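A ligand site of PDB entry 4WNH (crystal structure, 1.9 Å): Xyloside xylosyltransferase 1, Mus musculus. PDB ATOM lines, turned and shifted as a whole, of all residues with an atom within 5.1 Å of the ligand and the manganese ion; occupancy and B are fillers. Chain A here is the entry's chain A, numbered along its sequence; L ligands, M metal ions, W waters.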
ATOM      1  N   MET A  17     -24.271  18.062  21.417  1.00  0.00           N
ATOM      2  CA  MET A  17     -25.193  17.234  20.680  1.00  0.00           C
ATOM      3  C   MET A  17     -24.506  16.723  19.414  1.00  0.00           C
ATOM      4  O   MET A  17     -23.944  17.507  18.680  1.00  0.00           O
ATOM      5  CB  MET A  17     -26.399  18.057  20.269  1.00  0.00           C
ATOM      6  CG  MET A  17     -27.240  18.577  21.418  1.00  0.00           C
ATOM      7  SD  MET A  17     -28.121  17.186  22.130  1.00  0.00           S
ATOM      8  CE  MET A  17     -28.910  16.563  20.626  1.00  0.00           C
ATOM      9  N   PHE A  18     -24.549  15.414  19.169  1.00  0.00           N
ATOM     10  CA  PHE A  18     -23.926  14.845  17.975  1.00  0.00           C
ATOM     11  C   PHE A  18     -24.736  13.638  17.529  1.00  0.00           C
ATOM     12  O   PHE A  18     -24.441  12.502  17.883  1.00  0.00           O
ATOM     13  CB  PHE A  18     -22.475  14.465  18.239  1.00  0.00           C
ATOM     14  CG  PHE A  18     -21.692  14.129  16.999  1.00  0.00           C
ATOM     15  CD1 PHE A  18     -21.498  15.078  15.996  1.00  0.00           C
ATOM     16  CD2 PHE A  18     -21.158  12.869  16.803  1.00  0.00           C
ATOM     17  CE1 PHE A  18     -20.761  14.780  14.862  1.00  0.00           C
ATOM     18  CE2 PHE A  18     -20.434  12.555  15.667  1.00  0.00           C
ATOM     19  CZ  PHE A  18     -20.226  13.517  14.688  1.00  0.00           C
ATOM     20  N   THR A  19     -25.783  13.930  16.765  1.00  0.00           N
ATOM     21  CA  THR A  19     -26.760  12.942  16.344  1.00  0.00           C
ATOM     22  C   THR A  19     -26.887  12.944  14.817  1.00  0.00           C
ATOM     23  O   THR A  19     -26.651  13.968  14.169  1.00  0.00           O
ATOM     24  CB  THR A  19     -28.138  13.282  16.934  1.00  0.00           C
ATOM     25  OG1 THR A  19     -28.467  14.637  16.608  1.00  0.00           O
ATOM     26  CG2 THR A  19     -28.124  13.140  18.445  1.00  0.00           C
ATOM     27  N   LYS A  20     -27.298  11.803  14.282  1.00  0.00           N
ATOM     28  CA  LYS A  20     -27.503  11.631  12.841  1.00  0.00           C
ATOM     29  C   LYS A  20     -26.246  11.991  12.046  1.00  0.00           C
ATOM     30  O   LYS A  20     -26.337  12.548  10.955  1.00  0.00           O
ATOM     31  CB  LYS A  20     -28.698  12.453  12.348  1.00  0.00           C
ATOM     32  CG  LYS A  20     -29.974  12.365  13.168  1.00  0.00           C
ATOM     33  CD  LYS A  20     -30.554  10.953  13.163  1.00  0.00           C
ATOM     34  CE  LYS A  20     -31.887  10.900  13.905  1.00  0.00           C
ATOM     35  NZ  LYS A  20     -32.829  12.008  13.570  1.00  0.00           N
ATOM     36  N   ASN A  24     -23.319  12.081   7.141  1.00  0.00           N
ATOM     37  CA  ASN A  24     -23.562  13.518   7.173  1.00  0.00           C
ATOM     38  C   ASN A  24     -22.193  14.178   7.244  1.00  0.00           C
ATOM     39  O   ASN A  24     -21.703  14.572   8.319  1.00  0.00           O
ATOM     40  CB  ASN A  24     -24.427  13.904   8.356  1.00  0.00           C
ATOM     41  CG  ASN A  24     -24.800  15.373   8.371  1.00  0.00           C
ATOM     42  OD1 ASN A  24     -24.207  16.192   7.684  1.00  0.00           O
ATOM     43  ND2 ASN A  24     -25.773  15.710   9.183  1.00  0.00           N
ATOM     44  N   LEU A  27     -21.801  17.804   8.832  1.00  0.00           N
ATOM     45  CA  LEU A  27     -21.776  17.756  10.300  1.00  0.00           C
ATOM     46  C   LEU A  27     -20.454  17.246  10.861  1.00  0.00           C
ATOM     47  O   LEU A  27     -19.923  17.804  11.828  1.00  0.00           O
ATOM     48  CB  LEU A  27     -22.923  16.894  10.837  1.00  0.00           C
ATOM     49  CG  LEU A  27     -23.055  16.866  12.388  1.00  0.00           C
ATOM     50  CD1 LEU A  27     -23.327  18.252  12.952  1.00  0.00           C
ATOM     51  CD2 LEU A  27     -24.167  15.927  12.811  1.00  0.00           C
ATOM     52  N   LYS A  30     -17.831  19.955  10.531  1.00  0.00           N
ATOM     53  CA  LYS A  30     -18.020  20.979  11.565  1.00  0.00           C
ATOM     54  C   LYS A  30     -17.502  20.500  12.905  1.00  0.00           C
ATOM     55  O   LYS A  30     -16.759  21.212  13.610  1.00  0.00           O
ATOM     56  CB  LYS A  30     -19.500  21.307  11.716  1.00  0.00           C
ATOM     57  CG  LYS A  30     -20.021  22.165  10.603  1.00  0.00           C
ATOM     58  CD  LYS A  30     -21.536  22.158  10.624  1.00  0.00           C
ATOM     59  CE  LYS A  30     -22.069  23.219   9.699  1.00  0.00           C
ATOM     60  NZ  LYS A  30     -23.550  23.098   9.600  1.00  0.00           N
ATOM     61  N   PHE A 118     -34.248  18.678  21.674  1.00  0.00           N
ATOM     62  CA  PHE A 118     -33.860  20.085  21.477  1.00  0.00           C
ATOM     63  C   PHE A 118     -34.193  20.936  22.713  1.00  0.00           C
ATOM     64  O   PHE A 118     -33.875  22.113  22.752  1.00  0.00           O
ATOM     65  CB  PHE A 118     -34.477  20.667  20.204  1.00  0.00           C
ATOM     66  CG  PHE A 118     -34.143  19.865  18.960  1.00  0.00           C
ATOM     67  CD1 PHE A 118     -32.831  19.628  18.598  1.00  0.00           C
ATOM     68  CD2 PHE A 118     -35.158  19.318  18.190  1.00  0.00           C
ATOM     69  CE1 PHE A 118     -32.513  18.864  17.482  1.00  0.00           C
ATOM     70  CE2 PHE A 118     -34.859  18.569  17.054  1.00  0.00           C
ATOM     71  CZ  PHE A 118     -33.533  18.332  16.719  1.00  0.00           C
ATOM     72  N   LEU A 138     -22.483  23.209  24.187  1.00  0.00           N
ATOM     73  CA  LEU A 138     -21.881  23.877  23.026  1.00  0.00           C
ATOM     74  C   LEU A 138     -22.329  23.212  21.730  1.00  0.00           C
ATOM     75  O   LEU A 138     -22.384  21.974  21.630  1.00  0.00           O
ATOM     76  CB  LEU A 138     -20.360  23.833  23.111  1.00  0.00           C
ATOM     77  CG  LEU A 138     -19.715  24.432  24.366  1.00  0.00           C
ATOM     78  CD1 LEU A 138     -18.417  23.719  24.759  1.00  0.00           C
ATOM     79  CD2 LEU A 138     -19.489  25.918  24.186  1.00  0.00           C
ATOM     80  N   ASP A 139     -22.687  24.041  20.741  1.00  0.00           N
ATOM     81  CA  ASP A 139     -22.893  23.566  19.379  1.00  0.00           C
ATOM     82  C   ASP A 139     -21.597  23.027  18.783  1.00  0.00           C
ATOM     83  O   ASP A 139     -20.503  23.263  19.330  1.00  0.00           O
ATOM     84  CB  ASP A 139     -23.391  24.709  18.485  1.00  0.00           C
ATOM     85  CG  ASP A 139     -24.864  24.937  18.601  1.00  0.00           C
ATOM     86  OD1 ASP A 139     -25.486  24.365  19.527  1.00  0.00           O
ATOM     87  OD2 ASP A 139     -25.411  25.700  17.793  1.00  0.00           O
ATOM     88  N   LEU A 140     -21.724  22.286  17.683  1.00  0.00           N
ATOM     89  CA  LEU A 140     -20.555  21.746  17.011  1.00  0.00           C
ATOM     90  C   LEU A 140     -20.157  22.521  15.743  1.00  0.00           C
ATOM     91  O   LEU A 140     -19.126  22.213  15.116  1.00  0.00           O
ATOM     92  CB  LEU A 140     -20.718  20.240  16.757  1.00  0.00           C
ATOM     93  CG  LEU A 140     -20.350  19.371  17.980  1.00  0.00           C
ATOM     94  CD1 LEU A 140     -20.782  17.914  17.840  1.00  0.00           C
ATOM     95  CD2 LEU A 140     -18.875  19.429  18.279  1.00  0.00           C
ATOM     96  N   ASP A 141     -20.932  23.534  15.383  1.00  0.00           N
ATOM     97  CA  ASP A 141     -20.573  24.447  14.282  1.00  0.00           C
ATOM     98  C   ASP A 141     -19.865  25.695  14.816  1.00  0.00           C
ATOM     99  O   ASP A 141     -20.123  26.813  14.349  1.00  0.00           O
ATOM    100  CB  ASP A 141     -21.815  24.811  13.451  1.00  0.00           C
ATOM    101  CG  ASP A 141     -22.882  25.540  14.245  1.00  0.00           C
ATOM    102  OD1 ASP A 141     -22.904  25.422  15.494  1.00  0.00           O
ATOM    103  OD2 ASP A 141     -23.731  26.220  13.636  1.00  0.00           O
ATOM    104  N   ASN A 202     -29.215  33.283  21.880  1.00  0.00           N
ATOM    105  CA  ASN A 202     -28.755  32.224  20.987  1.00  0.00           C
ATOM    106  C   ASN A 202     -28.249  31.042  21.826  1.00  0.00           C
ATOM    107  O   ASN A 202     -27.495  31.243  22.765  1.00  0.00           O
ATOM    108  CB  ASN A 202     -27.641  32.736  20.055  1.00  0.00           C
ATOM    109  CG  ASN A 202     -27.247  31.728  18.982  1.00  0.00           C
ATOM    110  OD1 ASN A 202     -27.779  31.704  17.855  1.00  0.00           O
ATOM    111  ND2 ASN A 202     -26.332  30.874  19.331  1.00  0.00           N
ATOM    112  N   SER A 203     -28.632  29.829  21.461  1.00  0.00           N
ATOM    113  CA  SER A 203     -28.307  28.632  22.262  1.00  0.00           C
ATOM    114  C   SER A 203     -26.965  27.923  21.954  1.00  0.00           C
ATOM    115  O   SER A 203     -26.665  26.876  22.531  1.00  0.00           O
ATOM    116  CB  SER A 203     -29.429  27.614  22.107  1.00  0.00           C
ATOM    117  OG  SER A 203     -29.525  27.183  20.755  1.00  0.00           O
ATOM    118  N   LEU A 241     -37.140  26.788  17.254  1.00  0.00           N
ATOM    119  CA  LEU A 241     -35.752  26.651  17.650  1.00  0.00           C
ATOM    120  C   LEU A 241     -35.555  26.100  19.074  1.00  0.00           C
ATOM    121  O   LEU A 241     -34.439  26.138  19.596  1.00  0.00           O
ATOM    122  CB  LEU A 241     -34.992  27.976  17.441  1.00  0.00           C
ATOM    123  CG  LEU A 241     -35.084  28.514  16.001  1.00  0.00           C
ATOM    124  CD1 LEU A 241     -34.442  29.892  15.873  1.00  0.00           C
ATOM    125  CD2 LEU A 241     -34.451  27.534  15.036  1.00  0.00           C
ATOM    126  N   ASP A 243     -35.029  24.927  22.770  1.00  0.00           N
ATOM    127  CA  ASP A 243     -34.507  25.507  23.997  1.00  0.00           C
ATOM    128  C   ASP A 243     -34.232  27.015  23.863  1.00  0.00           C
ATOM    129  O   ASP A 243     -34.599  27.811  24.733  1.00  0.00           O
ATOM    130  CB  ASP A 243     -33.246  24.760  24.500  1.00  0.00           C
ATOM    131  CG  ASP A 243     -32.063  24.745  23.505  1.00  0.00           C
ATOM    132  OD1 ASP A 243     -32.203  25.111  22.321  1.00  0.00           O
ATOM    133  OD2 ASP A 243     -30.960  24.319  23.925  1.00  0.00           O
ATOM    134  N   GLN A 244     -33.650  27.397  22.739  1.00  0.00           N
ATOM    135  CA  GLN A 244     -33.350  28.813  22.457  1.00  0.00           C
ATOM    136  C   GLN A 244     -34.596  29.692  22.578  1.00  0.00           C
ATOM    137  O   GLN A 244     -34.531  30.784  23.143  1.00  0.00           O
ATOM    138  CB  GLN A 244     -32.757  28.939  21.057  1.00  0.00           C
ATOM    139  CG  GLN A 244     -32.148  30.302  20.803  1.00  0.00           C
ATOM    140  CD  GLN A 244     -31.592  30.428  19.423  1.00  0.00           C
ATOM    141  OE1 GLN A 244     -30.524  29.903  19.142  1.00  0.00           O
ATOM    142  NE2 GLN A 244     -32.327  31.111  18.543  1.00  0.00           N
ATOM    143  N   HIS A 296     -19.350  31.303  15.758  1.00  0.00           N
ATOM    144  CA  HIS A 296     -20.473  30.386  15.597  1.00  0.00           C
ATOM    145  C   HIS A 296     -20.979  30.517  14.177  1.00  0.00           C
ATOM    146  O   HIS A 296     -21.619  31.518  13.823  1.00  0.00           O
ATOM    147  CB  HIS A 296     -21.552  30.692  16.646  1.00  0.00           C
ATOM    148  CG  HIS A 296     -22.725  29.760  16.630  1.00  0.00           C
ATOM    149  ND1 HIS A 296     -23.855  29.978  17.409  1.00  0.00           N
ATOM    150  CD2 HIS A 296     -22.968  28.622  15.938  1.00  0.00           C
ATOM    151  CE1 HIS A 296     -24.718  29.000  17.196  1.00  0.00           C
ATOM    152  NE2 HIS A 296     -24.211  28.179  16.302  1.00  0.00           N
ATOM    153  N   ASN A 298     -23.444  29.557  12.436  1.00  0.00           N
ATOM    154  CA  ASN A 298     -24.837  29.122  12.385  1.00  0.00           C
ATOM    155  C   ASN A 298     -25.454  29.292  11.007  1.00  0.00           C
ATOM    156  O   ASN A 298     -24.884  29.957  10.144  1.00  0.00           O
ATOM    157  CB  ASN A 298     -25.710  29.664  13.551  1.00  0.00           C
ATOM    158  CG  ASN A 298     -25.807  31.187  13.641  1.00  0.00           C
ATOM    159  OD1 ASN A 298     -26.790  31.703  14.187  1.00  0.00           O
ATOM    160  ND2 ASN A 298     -24.820  31.913  13.166  1.00  0.00           N
ATOM    161  N   CYS A 299     -26.591  28.622  10.823  1.00  0.00           N
ATOM    162  CA  CYS A 299     -27.231  28.419   9.517  1.00  0.00           C
ATOM    163  C   CYS A 299     -26.203  28.079   8.436  1.00  0.00           C
ATOM    164  O   CYS A 299     -26.169  28.691   7.368  1.00  0.00           O
ATOM    165  CB  CYS A 299     -28.151  29.577   9.129  1.00  0.00           C
ATOM    166  SG  CYS A 299     -27.393  31.122   8.533  1.00  0.00           S
ATOM    167  N   ASN A 300     -25.371  27.080   8.726  1.00  0.00           N
ATOM    168  CA  ASN A 300     -24.387  26.573   7.784  1.00  0.00           C
ATOM    169  C   ASN A 300     -23.472  27.635   7.179  1.00  0.00           C
ATOM    170  O   ASN A 300     -23.053  27.493   6.030  1.00  0.00           O
ATOM    171  CB  ASN A 300     -25.098  25.825   6.658  1.00  0.00           C
ATOM    172  CG  ASN A 300     -25.877  24.649   7.157  1.00  0.00           C
ATOM    173  OD1 ASN A 300     -25.340  23.815   7.866  1.00  0.00           O
ATOM    174  ND2 ASN A 300     -27.129  24.572   6.808  1.00  0.00           N
HETATM  175  C1  LIG L   1     -30.265  26.964  15.211  1.00  0.00           C
HETATM  176  C2  LIG L   1     -30.800  27.405  16.583  1.00  0.00           C
HETATM  177  O1  LIG L   1     -29.960  28.458  17.117  1.00  0.00           O
HETATM  178  C3  LIG L   1     -30.941  26.187  17.518  1.00  0.00           C
HETATM  179  O2  LIG L   1     -31.536  26.445  18.802  1.00  0.00           O
HETATM  180  C4  LIG L   1     -31.857  25.166  16.824  1.00  0.00           C
HETATM  181  O3  LIG L   1     -32.028  24.005  17.655  1.00  0.00           O
HETATM  182  C5  LIG L   1     -31.305  24.776  15.440  1.00  0.00           C
HETATM  183  O4  LIG L   1     -31.121  25.951  14.633  1.00  0.00           O
HETATM  184  P1  LIG L   1     -27.757  26.481  14.258  1.00  0.00           P
HETATM  185  O5  LIG L   1     -28.145  27.207  12.987  1.00  0.00           O
HETATM  186  O6  LIG L   1     -26.481  26.790  15.026  1.00  0.00           O
HETATM  187  O7  LIG L   1     -28.920  26.471  15.371  1.00  0.00           O
HETATM  188  O8  LIG L   1     -27.882  24.938  13.830  1.00  0.00           O
HETATM  189  P2  LIG L   1     -26.787  23.780  14.043  1.00  0.00           P
HETATM  190  O9  LIG L   1     -26.526  23.178  12.679  1.00  0.00           O
HETATM  191  O10 LIG L   1     -25.656  24.223  14.912  1.00  0.00           O
HETATM  192  O11 LIG L   1     -27.675  22.775  14.916  1.00  0.00           O
HETATM  193  C6  LIG L   1     -27.614  22.791  16.354  1.00  0.00           C
HETATM  194  C7  LIG L   1     -26.564  21.832  16.936  1.00  0.00           C
HETATM  195  O12 LIG L   1     -27.182  20.564  17.162  1.00  0.00           O
HETATM  196  C8  LIG L   1     -25.322  21.514  16.094  1.00  0.00           C
HETATM  197  O13 LIG L   1     -24.245  22.406  16.371  1.00  0.00           O
HETATM  198  C9  LIG L   1     -24.973  20.088  16.492  1.00  0.00           C
HETATM  199  O14 LIG L   1     -24.182  20.042  17.696  1.00  0.00           O
HETATM  200  C10 LIG L   1     -26.321  19.479  16.782  1.00  0.00           C
HETATM  201  N1  LIG L   1     -26.886  18.764  15.626  1.00  0.00           N
HETATM  202  C11 LIG L   1     -27.664  19.380  14.730  1.00  0.00           C
HETATM  203  C12 LIG L   1     -26.628  17.378  15.473  1.00  0.00           C
HETATM  204  O15 LIG L   1     -25.929  16.751  16.290  1.00  0.00           O
HETATM  205  N2  LIG L   1     -27.152  16.697  14.432  1.00  0.00           N
HETATM  206  C13 LIG L   1     -27.932  17.327  13.534  1.00  0.00           C
HETATM  207  O16 LIG L   1     -28.399  16.682  12.602  1.00  0.00           O
HETATM  208  C14 LIG L   1     -28.207  18.678  13.665  1.00  0.00           C
HETATM  209 MN    MN M   1     -24.878  26.177  15.709  1.00  0.00          MN
HETATM  210  O   HOH W   1     -32.105  27.112  11.884  1.00  0.00           O
HETATM  211  O   HOH W   2     -24.485  20.683  20.673  1.00  0.00           O
HETATM  212  O   HOH W   3     -31.867  23.101  20.436  1.00  0.00           O
HETATM  213  O   HOH W   4     -24.900  25.462  11.160  1.00  0.00           O
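Three residues have an atom within 4 Å of the manganese ion: Asp 139, Asp 141 and His 296.
Leu 27 touches the ligand (CD2 to N2, 3.5 Å).
Asn 202 touches the ligand.
OD1 of Asp 243 touches O2 of the ligand, at 3.8 Å.
Asn 298 touches the ligand (CB to O6, 3.3 Å).
Hydrophobic or aromatic side chains that line the ligand: Met 17, Leu 27, Leu 140, Leu 241 and His 296.
15 residues have an atom within 4 Å of the ligand: Met 17, Phe 18, Thr 19, Leu 27, Asp 139, Leu 140, Asp 141, Asn 202, Ser 203, Leu 241, Asp 243, Gln 244, His 296, Asn 298 and Cys 299.
Water W3 lies within hydrogen-bond range of OD1 of Asp 243 (2.8 Å), O3 of the ligand (2.9 Å) and O of Phe 118 (3.2 Å).
Water W2 lies within hydrogen-bond range of O of Leu 138 (2.6 Å), N of Met 17 (2.7 Å) and O14 of the ligand (3.1 Å).
Water W4 lies within hydrogen-bond range of N of Asn 300, NZ of Lys 30 and O9 of the ligand.
The side-chain amide nitrogen of Asn 298 is in hydrogen-bond range of the backbone carbonyl oxygen of His 296 (3.3 Å).
The side-chain amide nitrogen (ND2) of Asn 202 lies within hydrogen-bond range of a ring nitrogen (ND1) of His 296 (3.3 Å).
The side-chain amide oxygen (OE1) of Gln 244 sits at hydrogen-bond distance from the backbone NH (N) of Ser 203 (3.0 Å).
The backbone NH (N) of Leu 27 is in hydrogen-bond range of the side-chain amide oxygen (OD1) of Asn 24 (3.1 Å).
The backbone carbonyl oxygen of Phe 118 is in hydrogen-bond range of the backbone NH of Asp 243, at 3.0 Å.
An oxygen (O1) of the ligand sits at hydrogen-bond distance from the side-chain amide oxygen (OE1) of Gln 244 (2.6 Å).
An oxygen (O14) of the ligand lies within hydrogen-bond range of the backbone carbonyl oxygen (O) of Met 17.
O15 of the ligand sits at hydrogen-bond distance from N of Thr 19 (2.9 Å).
A nitrogen (N2) of the ligand lies within hydrogen-bond range of the backbone carbonyl oxygen of Thr 19, at 2.8 Å.
The side-chain hydroxyl of Thr 19 sits at hydrogen-bond distance from a nitrogen (N2) of the ligand, 3.3 Å away.
An oxygen (O13) of the ligand lies within hydrogen-bond range of the backbone NH of Leu 140 (2.8 Å).
The side-chain hydroxyl (OG) of Ser 203 lies within hydrogen-bond range of an oxygen (O2) of the ligand.
N of Cys 299 lies within hydrogen-bond range of O5 of the ligand.
The backbone carbonyl oxygen (O) of Leu 241 is in hydrogen-bond range of an oxygen (O2) of the ligand (3.0 Å).
The backbone NH (N) of Phe 18 sits close to an oxygen (O15) of the ligand, at 3.5 Å.
The manganese ion is bound by O6 of the ligand (1.8 Å), OD1 of Asp 141 (2.1 Å), NE2 of His 296 (2.2 Å), OD2 of Asp 139 (2.2 Å), O10 of the ligand (2.2 Å) and OD2 of Asp 141 (2.4 Å).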
